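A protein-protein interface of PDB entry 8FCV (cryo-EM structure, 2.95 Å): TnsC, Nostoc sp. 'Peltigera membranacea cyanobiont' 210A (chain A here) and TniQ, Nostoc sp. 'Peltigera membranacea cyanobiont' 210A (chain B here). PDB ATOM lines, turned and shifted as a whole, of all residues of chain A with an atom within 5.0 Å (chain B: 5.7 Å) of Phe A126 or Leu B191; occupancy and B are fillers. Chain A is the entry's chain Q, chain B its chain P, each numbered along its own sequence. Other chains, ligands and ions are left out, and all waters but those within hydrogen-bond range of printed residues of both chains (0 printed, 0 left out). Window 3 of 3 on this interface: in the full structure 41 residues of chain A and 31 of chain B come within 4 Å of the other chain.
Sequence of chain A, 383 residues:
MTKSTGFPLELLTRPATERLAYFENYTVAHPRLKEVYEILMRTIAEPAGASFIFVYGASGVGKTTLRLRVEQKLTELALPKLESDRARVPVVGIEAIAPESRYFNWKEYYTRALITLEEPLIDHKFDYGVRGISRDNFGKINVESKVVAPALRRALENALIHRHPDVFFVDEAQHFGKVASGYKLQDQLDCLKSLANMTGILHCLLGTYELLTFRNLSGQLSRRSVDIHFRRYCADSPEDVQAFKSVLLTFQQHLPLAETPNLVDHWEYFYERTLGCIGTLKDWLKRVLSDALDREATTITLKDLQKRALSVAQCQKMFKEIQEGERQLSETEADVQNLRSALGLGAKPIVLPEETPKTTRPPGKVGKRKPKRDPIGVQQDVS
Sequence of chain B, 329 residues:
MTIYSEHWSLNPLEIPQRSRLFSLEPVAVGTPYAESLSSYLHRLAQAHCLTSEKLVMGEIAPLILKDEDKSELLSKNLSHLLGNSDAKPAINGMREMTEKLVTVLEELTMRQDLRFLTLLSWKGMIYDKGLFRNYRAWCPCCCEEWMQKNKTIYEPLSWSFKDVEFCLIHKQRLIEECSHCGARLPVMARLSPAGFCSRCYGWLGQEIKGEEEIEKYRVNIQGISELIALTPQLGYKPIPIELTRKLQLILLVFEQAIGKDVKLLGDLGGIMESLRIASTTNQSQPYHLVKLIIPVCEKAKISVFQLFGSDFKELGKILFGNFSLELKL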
ATOM      1  N   HIS A 124      -8.379  11.059   9.303  1.00  0.00           N
ATOM      2  CA  HIS A 124      -7.042  11.503   8.928  1.00  0.00           C
ATOM      3  C   HIS A 124      -6.044  11.228  10.047  1.00  0.00           C
ATOM      4  O   HIS A 124      -5.161  10.377   9.904  1.00  0.00           O
ATOM      5  CB  HIS A 124      -7.066  12.994   8.586  1.00  0.00           C
ATOM      6  CG  HIS A 124      -7.197  13.278   7.123  1.00  0.00           C
ATOM      7  ND1 HIS A 124      -6.348  14.125   6.447  1.00  0.00           N
ATOM      8  CD2 HIS A 124      -8.086  12.825   6.207  1.00  0.00           C
ATOM      9  CE1 HIS A 124      -6.707  14.182   5.177  1.00  0.00           C
ATOM     10  NE2 HIS A 124      -7.758  13.402   5.004  1.00  0.00           N
ATOM     11  N   LYS A 125      -6.196  11.938  11.167  1.00  0.00           N
ATOM     12  CA  LYS A 125      -5.444  11.704  12.398  1.00  0.00           C
ATOM     13  C   LYS A 125      -3.931  11.752  12.205  1.00  0.00           C
ATOM     14  O   LYS A 125      -3.442  12.100  11.125  1.00  0.00           O
ATOM     15  CB  LYS A 125      -5.850  10.363  13.014  1.00  0.00           C
ATOM     16  CG  LYS A 125      -6.638  10.500  14.310  1.00  0.00           C
ATOM     17  CD  LYS A 125      -7.436  11.799  14.333  1.00  0.00           C
ATOM     18  CE  LYS A 125      -7.910  12.142  15.733  1.00  0.00           C
ATOM     19  NZ  LYS A 125      -8.422  13.538  15.821  1.00  0.00           N
ATOM     20  N   PHE A 126      -3.190  11.411  13.260  1.00  0.00           N
ATOM     21  CA  PHE A 126      -1.735  11.314  13.256  1.00  0.00           C
ATOM     22  C   PHE A 126      -1.298  10.827  14.629  1.00  0.00           C
ATOM     23  O   PHE A 126      -2.033  10.956  15.612  1.00  0.00           O
ATOM     24  CB  PHE A 126      -1.060  12.653  12.930  1.00  0.00           C
ATOM     25  CG  PHE A 126       0.433  12.563  12.798  1.00  0.00           C
ATOM     26  CD1 PHE A 126       1.005  11.841  11.763  1.00  0.00           C
ATOM     27  CD2 PHE A 126       1.262  13.193  13.708  1.00  0.00           C
ATOM     28  CE1 PHE A 126       2.379  11.753  11.639  1.00  0.00           C
ATOM     29  CE2 PHE A 126       2.635  13.108  13.589  1.00  0.00           C
ATOM     30  CZ  PHE A 126       3.195  12.388  12.552  1.00  0.00           C
ATOM     31  N   ASP A 127      -0.090  10.268  14.689  1.00  0.00           N
ATOM     32  CA  ASP A 127       0.510   9.811  15.938  1.00  0.00           C
ATOM     33  C   ASP A 127       1.737  10.662  16.229  1.00  0.00           C
ATOM     34  O   ASP A 127       2.713  10.631  15.472  1.00  0.00           O
ATOM     35  CB  ASP A 127       0.887   8.330  15.865  1.00  0.00           C
ATOM     36  CG  ASP A 127       1.512   7.949  14.538  1.00  0.00           C
ATOM     37  OD1 ASP A 127       1.464   8.771  13.599  1.00  0.00           O
ATOM     38  OD2 ASP A 127       2.052   6.828  14.435  1.00  0.00           O
ATOM     39  N   TYR A 128       1.692  11.412  17.331  1.00  0.00           N
ATOM     40  CA  TYR A 128       2.776  12.317  17.710  1.00  0.00           C
ATOM     41  C   TYR A 128       3.840  11.541  18.490  1.00  0.00           C
ATOM     42  O   TYR A 128       4.009  11.680  19.702  1.00  0.00           O
ATOM     43  CB  TYR A 128       2.233  13.489  18.515  1.00  0.00           C
ATOM     44  CG  TYR A 128       1.723  14.630  17.665  1.00  0.00           C
ATOM     45  CD1 TYR A 128       0.568  14.495  16.906  1.00  0.00           C
ATOM     46  CD2 TYR A 128       2.393  15.845  17.627  1.00  0.00           C
ATOM     47  CE1 TYR A 128       0.097  15.536  16.130  1.00  0.00           C
ATOM     48  CE2 TYR A 128       1.929  16.892  16.854  1.00  0.00           C
ATOM     49  CZ  TYR A 128       0.782  16.731  16.109  1.00  0.00           C
ATOM     50  OH  TYR A 128       0.319  17.772  15.338  1.00  0.00           O
ATOM     51  N   ALA A 151      -2.448   6.131  17.764  1.00  0.00           N
ATOM     52  CA  ALA A 151      -2.889   7.489  17.464  1.00  0.00           C
ATOM     53  C   ALA A 151      -4.332   7.716  17.888  1.00  0.00           C
ATOM     54  O   ALA A 151      -4.649   8.741  18.501  1.00  0.00           O
ATOM     55  CB  ALA A 151      -2.720   7.778  15.973  1.00  0.00           C
ATOM     56  N   HIS B  42       0.111  24.954  16.781  1.00  0.00           N
ATOM     57  CA  HIS B  42       0.775  23.657  16.860  1.00  0.00           C
ATOM     58  C   HIS B  42       0.332  22.881  18.095  1.00  0.00           C
ATOM     59  O   HIS B  42       0.180  21.655  18.040  1.00  0.00           O
ATOM     60  CB  HIS B  42       2.291  23.838  16.838  1.00  0.00           C
ATOM     61  CG  HIS B  42       2.830  24.218  15.493  1.00  0.00           C
ATOM     62  ND1 HIS B  42       3.041  23.294  14.491  1.00  0.00           N
ATOM     63  CD2 HIS B  42       3.203  25.415  14.986  1.00  0.00           C
ATOM     64  CE1 HIS B  42       3.517  23.910  13.424  1.00  0.00           C
ATOM     65  NE2 HIS B  42       3.626  25.197  13.699  1.00  0.00           N
ATOM     66  N   CYS B  49      -4.202  15.284  17.905  1.00  0.00           N
ATOM     67  CA  CYS B  49      -3.471  14.218  17.214  1.00  0.00           C
ATOM     68  C   CYS B  49      -3.513  14.411  15.701  1.00  0.00           C
ATOM     69  O   CYS B  49      -3.628  13.453  14.933  1.00  0.00           O
ATOM     70  CB  CYS B  49      -3.991  12.836  17.611  1.00  0.00           C
ATOM     71  SG  CYS B  49      -3.507  12.328  19.272  1.00  0.00           S
ATOM     72  N   LEU B  50      -3.423  15.666  15.273  1.00  0.00           N
ATOM     73  CA  LEU B  50      -3.386  16.033  13.868  1.00  0.00           C
ATOM     74  C   LEU B  50      -2.188  16.939  13.634  1.00  0.00           C
ATOM     75  O   LEU B  50      -1.758  17.662  14.533  1.00  0.00           O
ATOM     76  CB  LEU B  50      -4.674  16.753  13.443  1.00  0.00           C
ATOM     77  CG  LEU B  50      -5.929  15.907  13.220  1.00  0.00           C
ATOM     78  CD1 LEU B  50      -7.175  16.763  13.373  1.00  0.00           C
ATOM     79  CD2 LEU B  50      -5.891  15.267  11.845  1.00  0.00           C
ATOM     80  N   THR B  51      -1.638  16.882  12.426  1.00  0.00           N
ATOM     81  CA  THR B  51      -0.594  17.829  12.069  1.00  0.00           C
ATOM     82  C   THR B  51      -1.196  19.221  11.918  1.00  0.00           C
ATOM     83  O   THR B  51      -2.380  19.377  11.610  1.00  0.00           O
ATOM     84  CB  THR B  51       0.105  17.411  10.775  1.00  0.00           C
ATOM     85  OG1 THR B  51      -0.658  17.860   9.650  1.00  0.00           O
ATOM     86  CG2 THR B  51       0.245  15.897  10.714  1.00  0.00           C
ATOM     87  N   SER B  52      -0.370  20.241  12.164  1.00  0.00           N
ATOM     88  CA  SER B  52      -0.845  21.615  12.034  1.00  0.00           C
ATOM     89  C   SER B  52      -1.382  21.873  10.634  1.00  0.00           C
ATOM     90  O   SER B  52      -2.455  22.462  10.470  1.00  0.00           O
ATOM     91  CB  SER B  52       0.281  22.592  12.372  1.00  0.00           C
ATOM     92  OG  SER B  52       0.815  22.330  13.658  1.00  0.00           O
ATOM     93  N   GLU B  53      -0.654  21.413   9.616  1.00  0.00           N
ATOM     94  CA  GLU B  53      -1.122  21.507   8.236  1.00  0.00           C
ATOM     95  C   GLU B  53      -2.486  20.842   8.062  1.00  0.00           C
ATOM     96  O   GLU B  53      -3.434  21.464   7.554  1.00  0.00           O
ATOM     97  CB  GLU B  53      -0.072  20.866   7.321  1.00  0.00           C
ATOM     98  CG  GLU B  53      -0.382  20.863   5.844  1.00  0.00           C
ATOM     99  CD  GLU B  53       0.804  21.270   4.989  1.00  0.00           C
ATOM    100  OE1 GLU B  53       1.799  21.784   5.540  1.00  0.00           O
ATOM    101  OE2 GLU B  53       0.745  21.063   3.760  1.00  0.00           O
ATOM    102  N   ALA B 189       4.943  25.052   9.167  1.00  0.00           N
ATOM    103  CA  ALA B 189       5.399  23.828   8.525  1.00  0.00           C
ATOM    104  C   ALA B 189       4.281  22.796   8.608  1.00  0.00           C
ATOM    105  O   ALA B 189       3.251  23.016   9.251  1.00  0.00           O
ATOM    106  CB  ALA B 189       6.689  23.311   9.169  1.00  0.00           C
ATOM    107  N   ARG B 190       4.497  21.662   7.939  1.00  0.00           N
ATOM    108  CA  ARG B 190       3.521  20.579   7.984  1.00  0.00           C
ATOM    109  C   ARG B 190       3.371  20.028   9.395  1.00  0.00           C
ATOM    110  O   ARG B 190       2.255  19.745   9.846  1.00  0.00           O
ATOM    111  CB  ARG B 190       3.927  19.474   7.010  1.00  0.00           C
ATOM    112  CG  ARG B 190       3.003  18.272   7.002  1.00  0.00           C
ATOM    113  CD  ARG B 190       3.473  17.239   5.996  1.00  0.00           C
ATOM    114  NE  ARG B 190       2.404  16.334   5.597  1.00  0.00           N
ATOM    115  CZ  ARG B 190       2.508  15.440   4.623  1.00  0.00           C
ATOM    116  NH1 ARG B 190       3.618  15.316   3.915  1.00  0.00           N
ATOM    117  NH2 ARG B 190       1.471  14.652   4.352  1.00  0.00           N
ATOM    118  N   LEU B 191       4.486  19.871  10.109  1.00  0.00           N
ATOM    119  CA  LEU B 191       4.458  19.362  11.479  1.00  0.00           C
ATOM    120  C   LEU B 191       5.649  19.970  12.213  1.00  0.00           C
ATOM    121  O   LEU B 191       6.783  19.504  12.054  1.00  0.00           O
ATOM    122  CB  LEU B 191       4.505  17.840  11.500  1.00  0.00           C
ATOM    123  CG  LEU B 191       4.694  17.190  12.871  1.00  0.00           C
ATOM    124  CD1 LEU B 191       3.546  17.554  13.796  1.00  0.00           C
ATOM    125  CD2 LEU B 191       4.832  15.683  12.737  1.00  0.00           C
ATOM    126  N   SER B 192       5.391  21.009  13.004  1.00  0.00           N
ATOM    127  CA  SER B 192       6.428  21.708  13.761  1.00  0.00           C
ATOM    128  C   SER B 192       5.974  21.892  15.205  1.00  0.00           C
ATOM    129  O   SER B 192       5.605  23.000  15.615  1.00  0.00           O
ATOM    130  CB  SER B 192       6.764  23.052  13.117  1.00  0.00           C
ATOM    131  OG  SER B 192       7.794  23.715  13.830  1.00  0.00           O
ATOM    132  N   PRO B 193       5.983  20.823  16.001  1.00  0.00           N
ATOM    133  CA  PRO B 193       5.684  20.977  17.429  1.00  0.00           C
ATOM    134  C   PRO B 193       6.730  21.847  18.107  1.00  0.00           C
ATOM    135  O   PRO B 193       7.898  21.872  17.714  1.00  0.00           O
ATOM    136  CB  PRO B 193       5.713  19.540  17.961  1.00  0.00           C
ATOM    137  CG  PRO B 193       6.515  18.774  16.971  1.00  0.00           C
ATOM    138  CD  PRO B 193       6.312  19.434  15.644  1.00  0.00           C
ATOM    139  N   CYS B 197      12.803  20.398  15.988  1.00  0.00           N
ATOM    140  CA  CYS B 197      13.231  20.835  14.666  1.00  0.00           C
ATOM    141  C   CYS B 197      12.173  20.444  13.642  1.00  0.00           C
ATOM    142  O   CYS B 197      11.864  19.260  13.482  1.00  0.00           O
ATOM    143  CB  CYS B 197      14.580  20.217  14.311  1.00  0.00           C
ATOM    144  SG  CYS B 197      15.056  20.421  12.581  1.00  0.00           S
ATOM    145  N   SER B 198      11.613  21.439  12.952  1.00  0.00           N
ATOM    146  CA  SER B 198      10.544  21.169  11.999  1.00  0.00           C
ATOM    147  C   SER B 198      11.017  20.354  10.803  1.00  0.00           C
ATOM    148  O   SER B 198      10.186  19.792  10.084  1.00  0.00           O
ATOM    149  CB  SER B 198       9.919  22.479  11.517  1.00  0.00           C
ATOM    150  OG  SER B 198      10.891  23.321  10.924  1.00  0.00           O
ATOM    151  N   TYR B 201      13.429  16.806  12.948  1.00  0.00           N
ATOM    152  CA  TYR B 201      12.787  16.257  14.139  1.00  0.00           C
ATOM    153  C   TYR B 201      13.761  16.173  15.311  1.00  0.00           C
ATOM    154  O   TYR B 201      13.471  15.529  16.324  1.00  0.00           O
ATOM    155  CB  TYR B 201      12.177  14.882  13.835  1.00  0.00           C
ATOM    156  CG  TYR B 201      11.138  14.420  14.831  1.00  0.00           C
ATOM    157  CD1 TYR B 201       9.889  15.025  14.894  1.00  0.00           C
ATOM    158  CD2 TYR B 201      11.398  13.365  15.699  1.00  0.00           C
ATOM    159  CE1 TYR B 201       8.934  14.602  15.801  1.00  0.00           C
ATOM    160  CE2 TYR B 201      10.449  12.936  16.608  1.00  0.00           C
ATOM    161  CZ  TYR B 201       9.219  13.557  16.654  1.00  0.00           C
ATOM    162  OH  TYR B 201       8.272  13.133  17.557  1.00  0.00           O
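Printed residues of chain B that touch a printed residue of chain A: Cys B49, Leu B50, Thr B51 and Leu B191. Hydrophobic or aromatic side chains of chain B within 4 Å of the printed part of chain A: Leu B50 and Leu B191. Along chain A the printed residues that touch a printed residue of chain B span positions 125 to 151. Among the printed residues, 10 pairs touch across the chains. Among the printed residues, no Asp or Glu carboxylate lies within 4 Å of a Lys or Arg side-chain nitrogen of the other chain.
Lys A125 touches Cys B49. Leu B50 touches Lys A125. Phe A126 touches Thr B51 (CG to CG2, 3.9 Å). Phe A126 touches Leu B191. CE1 of Tyr A128 touches C of Cys B49 (3.8 Å). Tyr A128 touches Thr B51 (OH to CA, 3.4 Å). CE2 of Tyr A128 touches CD1 of Leu B191, at 3.5 Å. O of Ala A151 touches SG of Cys B49, at 3.8 Å.
Printed residues of chain B within 4 Å of Phe A126: Cys B49, Thr B51 and Leu B191. Printed residues of chain B within 4 Å of Ala A151: Cys B49 (3.8 Å). Of the printed residues of chain A, Thr B51 touches Phe A126 and Tyr A128. Ala B189 touches none of the printed residues of chain A. Of the printed residues of chain A, Leu B191 touches Phe A126 and Tyr A128. The nearest residue of chain B that does not touch Phe A126 is Leu B50 (4.2 Å). The nearest printed residue of chain A that does not touch Leu B191 is Asp A127 (6.1 Å). The nearest printed residue of chain A that does not touch Cys B49 is Asp A127 (4.8 Å).
N of Phe A126 is in hydrogen-bond range of O of Cys B49 (2.7 Å). The side-chain hydroxyl of Tyr A128 lies close to the backbone carbonyl oxygen of Leu B50 (2.2 Å).
OG1 of Thr B51 sits close to O of Arg B190, at 3.5 Å.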
